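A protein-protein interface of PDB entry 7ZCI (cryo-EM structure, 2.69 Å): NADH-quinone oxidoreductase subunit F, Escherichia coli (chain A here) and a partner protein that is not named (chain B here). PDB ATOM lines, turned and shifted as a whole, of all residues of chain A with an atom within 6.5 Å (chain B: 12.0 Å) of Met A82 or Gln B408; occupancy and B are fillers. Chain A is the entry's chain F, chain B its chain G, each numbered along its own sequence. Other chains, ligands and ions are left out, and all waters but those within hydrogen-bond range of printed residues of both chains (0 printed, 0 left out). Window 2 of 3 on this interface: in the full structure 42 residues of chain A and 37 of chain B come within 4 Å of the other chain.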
ATOM      1  N   PRO A  77     -24.526 -18.087 -25.246  1.00  0.00           N
ATOM      2  CA  PRO A  77     -23.093 -18.326 -25.453  1.00  0.00           C
ATOM      3  C   PRO A  77     -22.681 -18.197 -26.909  1.00  0.00           C
ATOM      4  O   PRO A  77     -23.445 -18.491 -27.830  1.00  0.00           O
ATOM      5  CB  PRO A  77     -22.898 -19.762 -24.952  1.00  0.00           C
ATOM      6  CG  PRO A  77     -24.083 -20.044 -24.107  1.00  0.00           C
ATOM      7  CD  PRO A  77     -25.199 -19.288 -24.728  1.00  0.00           C
ATOM      8  N   ASP A  79     -20.267 -19.963 -28.088  1.00  0.00           N
ATOM      9  CA  ASP A  79     -19.724 -21.255 -28.472  1.00  0.00           C
ATOM     10  C   ASP A  79     -20.567 -21.859 -29.587  1.00  0.00           C
ATOM     11  O   ASP A  79     -21.784 -22.012 -29.448  1.00  0.00           O
ATOM     12  CB  ASP A  79     -19.699 -22.182 -27.256  1.00  0.00           C
ATOM     13  CG  ASP A  79     -18.703 -23.313 -27.395  1.00  0.00           C
ATOM     14  OD1 ASP A  79     -18.442 -23.761 -28.531  1.00  0.00           O
ATOM     15  OD2 ASP A  79     -18.178 -23.764 -26.356  1.00  0.00           O
ATOM     16  N   GLU A  80     -19.915 -22.213 -30.693  1.00  0.00           N
ATOM     17  CA  GLU A  80     -20.606 -22.821 -31.820  1.00  0.00           C
ATOM     18  C   GLU A  80     -20.884 -24.303 -31.617  1.00  0.00           C
ATOM     19  O   GLU A  80     -21.645 -24.884 -32.398  1.00  0.00           O
ATOM     20  CB  GLU A  80     -19.793 -22.621 -33.108  1.00  0.00           C
ATOM     21  CG  GLU A  80     -20.591 -22.423 -34.424  1.00  0.00           C
ATOM     22  CD  GLU A  80     -21.702 -21.362 -34.405  1.00  0.00           C
ATOM     23  OE1 GLU A  80     -22.487 -21.343 -35.377  1.00  0.00           O
ATOM     24  OE2 GLU A  80     -21.757 -20.490 -33.511  1.00  0.00           O
ATOM     25  N   SER A  81     -20.297 -24.925 -30.596  1.00  0.00           N
ATOM     26  CA  SER A  81     -20.584 -26.320 -30.289  1.00  0.00           C
ATOM     27  C   SER A  81     -21.909 -26.505 -29.559  1.00  0.00           C
ATOM     28  O   SER A  81     -22.346 -27.647 -29.385  1.00  0.00           O
ATOM     29  CB  SER A  81     -19.451 -26.923 -29.458  1.00  0.00           C
ATOM     30  OG  SER A  81     -19.287 -26.230 -28.236  1.00  0.00           O
ATOM     31  N   MET A  82     -22.547 -25.421 -29.125  1.00  0.00           N
ATOM     32  CA  MET A  82     -23.872 -25.465 -28.521  1.00  0.00           C
ATOM     33  C   MET A  82     -24.875 -25.014 -29.574  1.00  0.00           C
ATOM     34  O   MET A  82     -24.924 -23.832 -29.925  1.00  0.00           O
ATOM     35  CB  MET A  82     -23.935 -24.572 -27.286  1.00  0.00           C
ATOM     36  CG  MET A  82     -22.970 -24.954 -26.183  1.00  0.00           C
ATOM     37  SD  MET A  82     -22.971 -23.740 -24.853  1.00  0.00           S
ATOM     38  CE  MET A  82     -21.799 -24.465 -23.716  1.00  0.00           C
ATOM     39  N   ASN A  83     -25.664 -25.954 -30.086  1.00  0.00           N
ATOM     40  CA  ASN A  83     -26.658 -25.657 -31.112  1.00  0.00           C
ATOM     41  C   ASN A  83     -27.950 -26.413 -30.844  1.00  0.00           C
ATOM     42  O   ASN A  83     -28.645 -26.840 -31.770  1.00  0.00           O
ATOM     43  CB  ASN A  83     -26.117 -25.978 -32.503  1.00  0.00           C
ATOM     44  CG  ASN A  83     -25.382 -27.295 -32.545  1.00  0.00           C
ATOM     45  OD1 ASN A  83     -24.604 -27.613 -31.649  1.00  0.00           O
ATOM     46  ND2 ASN A  83     -25.629 -28.076 -33.587  1.00  0.00           N
ATOM     47  N   ILE A  84     -28.296 -26.577 -29.570  1.00  0.00           N
ATOM     48  CA  ILE A  84     -29.522 -27.254 -29.159  1.00  0.00           C
ATOM     49  C   ILE A  84     -30.374 -26.200 -28.458  1.00  0.00           C
ATOM     50  O   ILE A  84     -31.009 -26.458 -27.430  1.00  0.00           O
ATOM     51  CB  ILE A  84     -29.231 -28.484 -28.274  1.00  0.00           C
ATOM     52  CG1 ILE A  84     -28.139 -29.347 -28.897  1.00  0.00           C
ATOM     53  CG2 ILE A  84     -30.435 -29.410 -28.189  1.00  0.00           C
ATOM     54  CD1 ILE A  84     -28.467 -29.851 -30.288  1.00  0.00           C
ATOM     55  N   ARG A  85     -30.343 -24.981 -28.977  1.00  0.00           N
ATOM     56  CA  ARG A  85     -30.930 -23.849 -28.281  1.00  0.00           C
ATOM     57  C   ARG A  85     -32.457 -23.823 -28.365  1.00  0.00           C
ATOM     58  O   ARG A  85     -33.086 -24.257 -29.353  1.00  0.00           O
ATOM     59  CB  ARG A  85     -30.340 -22.552 -28.819  1.00  0.00           C
ATOM     60  CG  ARG A  85     -28.837 -22.593 -28.857  1.00  0.00           C
ATOM     61  CD  ARG A  85     -28.225 -21.250 -29.120  1.00  0.00           C
ATOM     62  NE  ARG A  85     -26.791 -21.296 -28.876  1.00  0.00           N
ATOM     63  CZ  ARG A  85     -25.994 -20.239 -28.879  1.00  0.00           C
ATOM     64  NH1 ARG A  85     -26.461 -19.022 -29.101  1.00  0.00           N
ATOM     65  NH2 ARG A  85     -24.696 -20.406 -28.649  1.00  0.00           N
ATOM     66  N   LYS A 124     -30.603 -18.410 -32.816  1.00  0.00           N
ATOM     67  CA  LYS A 124     -30.192 -19.690 -33.394  1.00  0.00           C
ATOM     68  C   LYS A 124     -30.847 -20.859 -32.670  1.00  0.00           C
ATOM     69  O   LYS A 124     -30.256 -21.928 -32.523  1.00  0.00           O
ATOM     70  CB  LYS A 124     -28.666 -19.837 -33.411  1.00  0.00           C
ATOM     71  CG  LYS A 124     -27.966 -18.803 -34.267  1.00  0.00           C
ATOM     72  CD  LYS A 124     -26.461 -18.944 -34.201  1.00  0.00           C
ATOM     73  CE  LYS A 124     -25.912 -18.373 -32.910  1.00  0.00           C
ATOM     74  NZ  LYS A 124     -26.137 -16.907 -32.828  1.00  0.00           N
ATOM     75  N   PRO A 202     -26.408 -19.870 -12.506  1.00  0.00           N
ATOM     76  CA  PRO A 202     -26.457 -19.560 -13.942  1.00  0.00           C
ATOM     77  C   PRO A 202     -27.839 -19.199 -14.466  1.00  0.00           C
ATOM     78  O   PRO A 202     -28.840 -19.803 -14.099  1.00  0.00           O
ATOM     79  CB  PRO A 202     -25.963 -20.851 -14.587  1.00  0.00           C
ATOM     80  CG  PRO A 202     -26.342 -21.901 -13.636  1.00  0.00           C
ATOM     81  CD  PRO A 202     -26.214 -21.309 -12.272  1.00  0.00           C
ATOM     82  N   THR A 206     -27.417 -19.365 -20.473  1.00  0.00           N
ATOM     83  CA  THR A 206     -26.276 -20.266 -20.553  1.00  0.00           C
ATOM     84  C   THR A 206     -26.631 -21.709 -20.228  1.00  0.00           C
ATOM     85  O   THR A 206     -26.106 -22.628 -20.860  1.00  0.00           O
ATOM     86  CB  THR A 206     -25.158 -19.797 -19.620  1.00  0.00           C
ATOM     87  OG1 THR A 206     -25.620 -19.812 -18.265  1.00  0.00           O
ATOM     88  CG2 THR A 206     -24.725 -18.396 -19.985  1.00  0.00           C
ATOM     89  N   SER A 207     -27.509 -21.932 -19.253  1.00  0.00           N
ATOM     90  CA  SER A 207     -27.906 -23.277 -18.838  1.00  0.00           C
ATOM     91  C   SER A 207     -29.391 -23.226 -18.496  1.00  0.00           C
ATOM     92  O   SER A 207     -29.767 -22.901 -17.368  1.00  0.00           O
ATOM     93  CB  SER A 207     -27.072 -23.758 -17.661  1.00  0.00           C
ATOM     94  OG  SER A 207     -27.501 -25.034 -17.233  1.00  0.00           O
ATOM     95  N   GLY A 211     -30.390 -28.053 -19.700  1.00  0.00           N
ATOM     96  CA  GLY A 211     -29.010 -27.629 -19.651  1.00  0.00           C
ATOM     97  C   GLY A 211     -28.523 -26.865 -20.858  1.00  0.00           C
ATOM     98  O   GLY A 211     -27.351 -26.474 -20.886  1.00  0.00           O
ATOM     99  N   PRO A 213     -28.658 -23.657 -23.805  1.00  0.00           N
ATOM    100  CA  PRO A 213     -29.048 -22.246 -23.891  1.00  0.00           C
ATOM    101  C   PRO A 213     -30.530 -22.091 -24.205  1.00  0.00           C
ATOM    102  O   PRO A 213     -31.053 -22.653 -25.174  1.00  0.00           O
ATOM    103  CB  PRO A 213     -28.160 -21.698 -25.014  1.00  0.00           C
ATOM    104  CG  PRO A 213     -27.315 -22.841 -25.481  1.00  0.00           C
ATOM    105  CD  PRO A 213     -27.356 -23.892 -24.443  1.00  0.00           C
ATOM    106  N   GLY B 399     -19.676 -38.020 -11.507  1.00  0.00           N
ATOM    107  CA  GLY B 399     -18.500 -37.219 -11.827  1.00  0.00           C
ATOM    108  C   GLY B 399     -18.501 -36.549 -13.191  1.00  0.00           C
ATOM    109  O   GLY B 399     -17.892 -35.490 -13.357  1.00  0.00           O
ATOM    110  N   LYS B 400     -19.166 -37.142 -14.189  1.00  0.00           N
ATOM    111  CA  LYS B 400     -19.165 -36.534 -15.519  1.00  0.00           C
ATOM    112  C   LYS B 400     -19.958 -35.234 -15.547  1.00  0.00           C
ATOM    113  O   LYS B 400     -19.529 -34.252 -16.163  1.00  0.00           O
ATOM    114  CB  LYS B 400     -19.723 -37.489 -16.568  1.00  0.00           C
ATOM    115  CG  LYS B 400     -19.589 -36.900 -17.964  1.00  0.00           C
ATOM    116  CD  LYS B 400     -20.230 -37.727 -19.038  1.00  0.00           C
ATOM    117  CE  LYS B 400     -19.938 -37.122 -20.401  1.00  0.00           C
ATOM    118  NZ  LYS B 400     -20.450 -37.968 -21.510  1.00  0.00           N
ATOM    119  N   ALA B 401     -21.125 -35.219 -14.902  1.00  0.00           N
ATOM    120  CA  ALA B 401     -21.877 -33.979 -14.764  1.00  0.00           C
ATOM    121  C   ALA B 401     -21.092 -32.959 -13.958  1.00  0.00           C
ATOM    122  O   ALA B 401     -21.140 -31.755 -14.253  1.00  0.00           O
ATOM    123  CB  ALA B 401     -23.227 -34.253 -14.107  1.00  0.00           C
ATOM    124  N   ARG B 402     -20.351 -33.425 -12.945  1.00  0.00           N
ATOM    125  CA  ARG B 402     -19.496 -32.503 -12.195  1.00  0.00           C
ATOM    126  C   ARG B 402     -18.444 -31.850 -13.093  1.00  0.00           C
ATOM    127  O   ARG B 402     -18.227 -30.634 -13.019  1.00  0.00           O
ATOM    128  CB  ARG B 402     -18.831 -33.233 -11.033  1.00  0.00           C
ATOM    129  CG  ARG B 402     -19.788 -33.582  -9.927  1.00  0.00           C
ATOM    130  CD  ARG B 402     -19.070 -33.916  -8.644  1.00  0.00           C
ATOM    131  NE  ARG B 402     -18.344 -35.176  -8.713  1.00  0.00           N
ATOM    132  CZ  ARG B 402     -18.889 -36.367  -8.517  1.00  0.00           C
ATOM    133  NH1 ARG B 402     -20.186 -36.510  -8.308  1.00  0.00           N
ATOM    134  NH2 ARG B 402     -18.113 -37.445  -8.530  1.00  0.00           N
ATOM    135  N   GLU B 403     -17.805 -32.635 -13.964  1.00  0.00           N
ATOM    136  CA  GLU B 403     -16.809 -32.084 -14.886  1.00  0.00           C
ATOM    137  C   GLU B 403     -17.440 -31.140 -15.902  1.00  0.00           C
ATOM    138  O   GLU B 403     -16.856 -30.099 -16.235  1.00  0.00           O
ATOM    139  CB  GLU B 403     -16.075 -33.208 -15.611  1.00  0.00           C
ATOM    140  CG  GLU B 403     -15.271 -34.120 -14.711  1.00  0.00           C
ATOM    141  CD  GLU B 403     -14.794 -35.363 -15.431  1.00  0.00           C
ATOM    142  OE1 GLU B 403     -15.406 -35.723 -16.457  1.00  0.00           O
ATOM    143  OE2 GLU B 403     -13.805 -35.976 -14.978  1.00  0.00           O
ATOM    144  N   MET B 404     -18.624 -31.496 -16.410  1.00  0.00           N
ATOM    145  CA  MET B 404     -19.315 -30.654 -17.383  1.00  0.00           C
ATOM    146  C   MET B 404     -19.671 -29.303 -16.785  1.00  0.00           C
ATOM    147  O   MET B 404     -19.533 -28.268 -17.443  1.00  0.00           O
ATOM    148  CB  MET B 404     -20.577 -31.352 -17.882  1.00  0.00           C
ATOM    149  CG  MET B 404     -20.377 -32.264 -19.064  1.00  0.00           C
ATOM    150  SD  MET B 404     -21.808 -33.316 -19.347  1.00  0.00           S
ATOM    151  CE  MET B 404     -22.949 -32.140 -20.057  1.00  0.00           C
ATOM    152  N   ALA B 405     -20.128 -29.296 -15.533  1.00  0.00           N
ATOM    153  CA  ALA B 405     -20.462 -28.037 -14.882  1.00  0.00           C
ATOM    154  C   ALA B 405     -19.220 -27.251 -14.501  1.00  0.00           C
ATOM    155  O   ALA B 405     -19.260 -26.018 -14.477  1.00  0.00           O
ATOM    156  CB  ALA B 405     -21.316 -28.299 -13.651  1.00  0.00           C
ATOM    157  N   ALA B 406     -18.121 -27.936 -14.184  1.00  0.00           N
ATOM    158  CA  ALA B 406     -16.867 -27.230 -13.950  1.00  0.00           C
ATOM    159  C   ALA B 406     -16.354 -26.574 -15.222  1.00  0.00           C
ATOM    160  O   ALA B 406     -15.677 -25.543 -15.155  1.00  0.00           O
ATOM    161  CB  ALA B 406     -15.818 -28.186 -13.388  1.00  0.00           C
ATOM    162  N   ALA B 407     -16.670 -27.150 -16.383  1.00  0.00           N
ATOM    163  CA  ALA B 407     -16.274 -26.543 -17.649  1.00  0.00           C
ATOM    164  C   ALA B 407     -17.004 -25.235 -17.929  1.00  0.00           C
ATOM    165  O   ALA B 407     -16.498 -24.415 -18.699  1.00  0.00           O
ATOM    166  CB  ALA B 407     -16.509 -27.525 -18.795  1.00  0.00           C
ATOM    167  N   GLN B 408     -18.169 -25.014 -17.319  1.00  0.00           N
ATOM    168  CA  GLN B 408     -18.937 -23.791 -17.503  1.00  0.00           C
ATOM    169  C   GLN B 408     -18.750 -22.802 -16.359  1.00  0.00           C
ATOM    170  O   GLN B 408     -19.538 -21.858 -16.238  1.00  0.00           O
ATOM    171  CB  GLN B 408     -20.421 -24.110 -17.668  1.00  0.00           C
ATOM    172  CG  GLN B 408     -20.768 -24.828 -18.948  1.00  0.00           C
ATOM    173  CD  GLN B 408     -22.209 -24.621 -19.340  1.00  0.00           C
ATOM    174  OE1 GLN B 408     -22.891 -23.758 -18.796  1.00  0.00           O
ATOM    175  NE2 GLN B 408     -22.686 -25.417 -20.283  1.00  0.00           N
ATOM    176  N   LYS B 409     -17.727 -23.012 -15.523  1.00  0.00           N
ATOM    177  CA  LYS B 409     -17.405 -22.159 -14.373  1.00  0.00           C
ATOM    178  C   LYS B 409     -18.564 -22.081 -13.380  1.00  0.00           C
ATOM    179  O   LYS B 409     -18.847 -21.028 -12.809  1.00  0.00           O
ATOM    180  CB  LYS B 409     -16.964 -20.764 -14.818  1.00  0.00           C
ATOM    181  CG  LYS B 409     -15.764 -20.768 -15.744  1.00  0.00           C
ATOM    182  CD  LYS B 409     -15.108 -19.402 -15.800  1.00  0.00           C
ATOM    183  CE  LYS B 409     -14.021 -19.263 -14.754  1.00  0.00           C
ATOM    184  NZ  LYS B 409     -13.425 -17.899 -14.752  1.00  0.00           N
ATOM    185  N   VAL B 410     -19.234 -23.206 -13.174  1.00  0.00           N
ATOM    186  CA  VAL B 410     -20.242 -23.340 -12.130  1.00  0.00           C
ATOM    187  C   VAL B 410     -19.566 -23.915 -10.893  1.00  0.00           C
ATOM    188  O   VAL B 410     -18.857 -24.924 -10.980  1.00  0.00           O
ATOM    189  CB  VAL B 410     -21.403 -24.235 -12.595  1.00  0.00           C
ATOM    190  CG1 VAL B 410     -22.306 -24.592 -11.435  1.00  0.00           C
ATOM    191  CG2 VAL B 410     -22.187 -23.547 -13.684  1.00  0.00           C
ATOM    192  N   ALA B 411     -19.776 -23.266  -9.749  1.00  0.00           N
ATOM    193  CA  ALA B 411     -19.136 -23.679  -8.506  1.00  0.00           C
ATOM    194  C   ALA B 411     -19.606 -25.066  -8.084  1.00  0.00           C
ATOM    195  O   ALA B 411     -20.757 -25.448  -8.301  1.00  0.00           O
ATOM    196  CB  ALA B 411     -19.429 -22.669  -7.403  1.00  0.00           C
ATOM    197  N   ASP B 412     -18.695 -25.821  -7.467  1.00  0.00           N
ATOM    198  CA  ASP B 412     -18.932 -27.240  -7.226  1.00  0.00           C
ATOM    199  C   ASP B 412     -19.948 -27.505  -6.125  1.00  0.00           C
ATOM    200  O   ASP B 412     -20.453 -28.626  -6.029  1.00  0.00           O
ATOM    201  CB  ASP B 412     -17.619 -27.941  -6.892  1.00  0.00           C
ATOM    202  CG  ASP B 412     -16.750 -27.135  -5.959  1.00  0.00           C
ATOM    203  OD1 ASP B 412     -16.944 -27.225  -4.731  1.00  0.00           O
ATOM    204  OD2 ASP B 412     -15.867 -26.407  -6.454  1.00  0.00           O
ATOM    205  N   TRP B 413     -20.261 -26.518  -5.295  1.00  0.00           N
ATOM    206  CA  TRP B 413     -21.302 -26.687  -4.295  1.00  0.00           C
ATOM    207  C   TRP B 413     -22.692 -26.392  -4.832  1.00  0.00           C
ATOM    208  O   TRP B 413     -23.677 -26.741  -4.180  1.00  0.00           O
ATOM    209  CB  TRP B 413     -21.025 -25.795  -3.086  1.00  0.00           C
ATOM    210  CG  TRP B 413     -20.517 -24.438  -3.435  1.00  0.00           C
ATOM    211  CD1 TRP B 413     -19.224 -24.026  -3.424  1.00  0.00           C
ATOM    212  CD2 TRP B 413     -21.294 -23.308  -3.830  1.00  0.00           C
ATOM    213  NE1 TRP B 413     -19.143 -22.710  -3.787  1.00  0.00           N
ATOM    214  CE2 TRP B 413     -20.404 -22.244  -4.042  1.00  0.00           C
ATOM    215  CE3 TRP B 413     -22.657 -23.091  -4.030  1.00  0.00           C
ATOM    216  CZ2 TRP B 413     -20.828 -20.991  -4.449  1.00  0.00           C
ATOM    217  CZ3 TRP B 413     -23.075 -21.851  -4.422  1.00  0.00           C
ATOM    218  CH2 TRP B 413     -22.167 -20.813  -4.631  1.00  0.00           C
ATOM    219  N   GLN B 414     -22.794 -25.774  -6.005  1.00  0.00           N
ATOM    220  CA  GLN B 414     -24.080 -25.403  -6.589  1.00  0.00           C
ATOM    221  C   GLN B 414     -24.641 -26.618  -7.319  1.00  0.00           C
ATOM    222  O   GLN B 414     -24.592 -26.726  -8.542  1.00  0.00           O
ATOM    223  CB  GLN B 414     -23.918 -24.210  -7.517  1.00  0.00           C
ATOM    224  CG  GLN B 414     -25.214 -23.500  -7.819  1.00  0.00           C
ATOM    225  CD  GLN B 414     -24.996 -22.127  -8.394  1.00  0.00           C
ATOM    226  OE1 GLN B 414     -23.865 -21.662  -8.504  1.00  0.00           O
ATOM    227  NE2 GLN B 414     -26.082 -21.468  -8.772  1.00  0.00           N
ATOM    228  N   ILE B 415     -25.212 -27.531  -6.534  1.00  0.00           N
ATOM    229  CA  ILE B 415     -25.506 -28.879  -7.009  1.00  0.00           C
ATOM    230  C   ILE B 415     -26.626 -28.878  -8.049  1.00  0.00           C
ATOM    231  O   ILE B 415     -26.586 -29.646  -9.016  1.00  0.00           O
ATOM    232  CB  ILE B 415     -25.812 -29.797  -5.809  1.00  0.00           C
ATOM    233  CG1 ILE B 415     -26.220 -31.195  -6.263  1.00  0.00           C
ATOM    234  CG2 ILE B 415     -26.856 -29.189  -4.896  1.00  0.00           C
ATOM    235  CD1 ILE B 415     -25.139 -31.918  -7.001  1.00  0.00           C
ATOM    236  N   ALA B 416     -27.632 -28.014  -7.881  1.00  0.00           N
ATOM    237  CA  ALA B 416     -28.768 -28.000  -8.801  1.00  0.00           C
ATOM    238  C   ALA B 416     -28.354 -27.566 -10.203  1.00  0.00           C
ATOM    239  O   ALA B 416     -28.817 -28.135 -11.196  1.00  0.00           O
ATOM    240  CB  ALA B 416     -29.867 -27.096  -8.256  1.00  0.00           C
ATOM    241  N   ALA B 417     -27.461 -26.579 -10.300  1.00  0.00           N
ATOM    242  CA  ALA B 417     -26.924 -26.183 -11.597  1.00  0.00           C
ATOM    243  C   ALA B 417     -26.094 -27.294 -12.227  1.00  0.00           C
ATOM    244  O   ALA B 417     -26.159 -27.504 -13.442  1.00  0.00           O
ATOM    245  CB  ALA B 417     -26.090 -24.918 -11.453  1.00  0.00           C
ATOM    246  N   ILE B 418     -25.306 -28.007 -11.418  1.00  0.00           N
ATOM    247  CA  ILE B 418     -24.493 -29.112 -11.923  1.00  0.00           C
ATOM    248  C   ILE B 418     -25.378 -30.212 -12.493  1.00  0.00           C
ATOM    249  O   ILE B 418     -25.151 -30.704 -13.604  1.00  0.00           O
ATOM    250  CB  ILE B 418     -23.582 -29.653 -10.807  1.00  0.00           C
ATOM    251  CG1 ILE B 418     -22.637 -28.569 -10.304  1.00  0.00           C
ATOM    252  CG2 ILE B 418     -22.809 -30.868 -11.282  1.00  0.00           C
ATOM    253  CD1 ILE B 418     -21.852 -28.978  -9.104  1.00  0.00           C
ATOM    254  N   LEU B 419     -26.415 -30.594 -11.747  1.00  0.00           N
ATOM    255  CA  LEU B 419     -27.328 -31.630 -12.212  1.00  0.00           C
ATOM    256  C   LEU B 419     -28.142 -31.173 -13.415  1.00  0.00           C
ATOM    257  O   LEU B 419     -28.506 -31.999 -14.256  1.00  0.00           O
ATOM    258  CB  LEU B 419     -28.256 -32.064 -11.081  1.00  0.00           C
ATOM    259  CG  LEU B 419     -27.624 -32.698  -9.841  1.00  0.00           C
ATOM    260  CD1 LEU B 419     -28.692 -33.056  -8.838  1.00  0.00           C
ATOM    261  CD2 LEU B 419     -26.825 -33.923 -10.215  1.00  0.00           C
ATOM    262  N   ASN B 420     -28.434 -29.875 -13.523  1.00  0.00           N
ATOM    263  CA  ASN B 420     -29.129 -29.383 -14.708  1.00  0.00           C
ATOM    264  C   ASN B 420     -28.231 -29.407 -15.935  1.00  0.00           C
ATOM    265  O   ASN B 420     -28.690 -29.724 -17.037  1.00  0.00           O
ATOM    266  CB  ASN B 420     -29.655 -27.971 -14.473  1.00  0.00           C
ATOM    267  CG  ASN B 420     -30.400 -27.432 -15.669  1.00  0.00           C
ATOM    268  OD1 ASN B 420     -29.974 -26.475 -16.302  1.00  0.00           O
ATOM    269  ND2 ASN B 420     -31.511 -28.067 -16.003  1.00  0.00           N
ATOM    270  N   ILE B 421     -26.961 -29.032 -15.774  1.00  0.00           N
ATOM    271  CA  ILE B 421     -26.022 -29.044 -16.891  1.00  0.00           C
ATOM    272  C   ILE B 421     -25.776 -30.470 -17.364  1.00  0.00           C
ATOM    273  O   ILE B 421     -25.875 -30.773 -18.558  1.00  0.00           O
ATOM    274  CB  ILE B 421     -24.712 -28.346 -16.489  1.00  0.00           C
ATOM    275  CG1 ILE B 421     -24.908 -26.832 -16.466  1.00  0.00           C
ATOM    276  CG2 ILE B 421     -23.587 -28.722 -17.422  1.00  0.00           C
ATOM    277  CD1 ILE B 421     -23.701 -26.062 -16.040  1.00  0.00           C
ATOM    278  N   GLY B 422     -25.457 -31.363 -16.437  1.00  0.00           N
ATOM    279  CA  GLY B 422     -25.270 -32.759 -16.760  1.00  0.00           C
ATOM    280  C   GLY B 422     -26.541 -33.562 -16.621  1.00  0.00           C
ATOM    281  O   GLY B 422     -26.706 -34.270 -15.624  1.00  0.00           O
ATOM    282  N   GLN B 423     -27.451 -33.442 -17.589  1.00  0.00           N
ATOM    283  CA  GLN B 423     -28.810 -33.967 -17.478  1.00  0.00           C
ATOM    284  C   GLN B 423     -28.871 -35.465 -17.223  1.00  0.00           C
ATOM    285  O   GLN B 423     -29.241 -35.903 -16.133  1.00  0.00           O
ATOM    286  CB  GLN B 423     -29.581 -33.665 -18.760  1.00  0.00           C
ATOM    287  CG  GLN B 423     -30.015 -32.239 -18.894  1.00  0.00           C
ATOM    288  CD  GLN B 423     -31.205 -31.934 -18.034  1.00  0.00           C
ATOM    289  OE1 GLN B 423     -32.154 -32.709 -17.982  1.00  0.00           O
ATOM    290  NE2 GLN B 423     -31.170 -30.797 -17.356  1.00  0.00           N
ATOM    291  N   ALA B 425     -26.082 -37.316 -18.696  1.00  0.00           N
ATOM    292  CA  ALA B 425     -24.715 -37.710 -18.975  1.00  0.00           C
ATOM    293  C   ALA B 425     -24.073 -38.286 -17.727  1.00  0.00           C
ATOM    294  O   ALA B 425     -24.294 -37.802 -16.615  1.00  0.00           O
ATOM    295  CB  ALA B 425     -23.911 -36.515 -19.476  1.00  0.00           C
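The side-chain amide oxygen (OD1) of Asn B420 lies within hydrogen-bond range of the side-chain hydroxyl (OG) of Ser A207 (3.0 Å).
NE of Arg A85 sits at hydrogen-bond distance from O of Met A82, at 3.3 Å.
The backbone carbonyl oxygen of Asn B420 lies within hydrogen-bond range of the side-chain amide nitrogen of Gln B423 (2.7 Å).
Among the printed residues, merely in contact across the chains: Ser A207 with Ile B421 (3.2 Å), Gly A211 with Asn B420 (3.4 Å), Pro A202 with Gln B414 (3.5 Å), Met A82 with Gln B408 (3.7 Å), Gly A211 with Gln B423 (3.7 Å), Pro A202 with Ala B417 (3.7 Å) and Thr A206 with Gln B408 (3.98 Å).
No residue of chain B comes within 4 Å of Pro A77.
No residue of chain B comes within 4 Å of Asp A79.
Glu A80 touches none of the printed residues of chain B.
No residue of chain B comes within 4 Å of Ser A81.
Met A82 touches one residue of chain B.
No residue of chain B comes within 4 Å of Asn A83.
No residue of chain B comes within 4 Å of Ile A84.
Of the printed residues of chain B, Pro A202 touches Gln B414 (3.5 Å) and Ala B417 (3.7 Å).
Printed residues of chain B within 4 Å of Thr A206: Gln B408 (3.98 Å).
Of chain B, only Asn B420 (3.0 Å) and Ile B421 (3.2 Å) come within 4 Å of Ser A207.
Of the printed residues of chain B, Gly A211 touches Asn B420 (3.4 Å) and Gln B423 (3.7 Å).
Of the printed residues of chain A, Gln B408 touches Met A82 and Thr A206.
Printed residues of chain A within 4 Å of Asn B420: Ser A207 and Gly A211.
Printed residues of chain A within 4 Å of Ile B421: Ser A207 (3.2 Å).
The nearest residue of chain B that does not touch Met A82 is Ala B407 (7.3 Å).
Of the 26 printed residues of chain B, 6 touch a printed residue of chain A.
Hydrophobic or aromatic side chains of chain B that line the printed part of chain A: Ala B417 and Ile B421.
Hydrophobic or aromatic side chains of chain A within 4 Å of the printed part of chain B: Met A82 and Pro A202.
Among the printed residues, 8 pairs touch across the chains.
Among the printed residues, no Asp or Glu carboxylate lies within 4 Å of a Lys or Arg side-chain nitrogen of the other chain.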
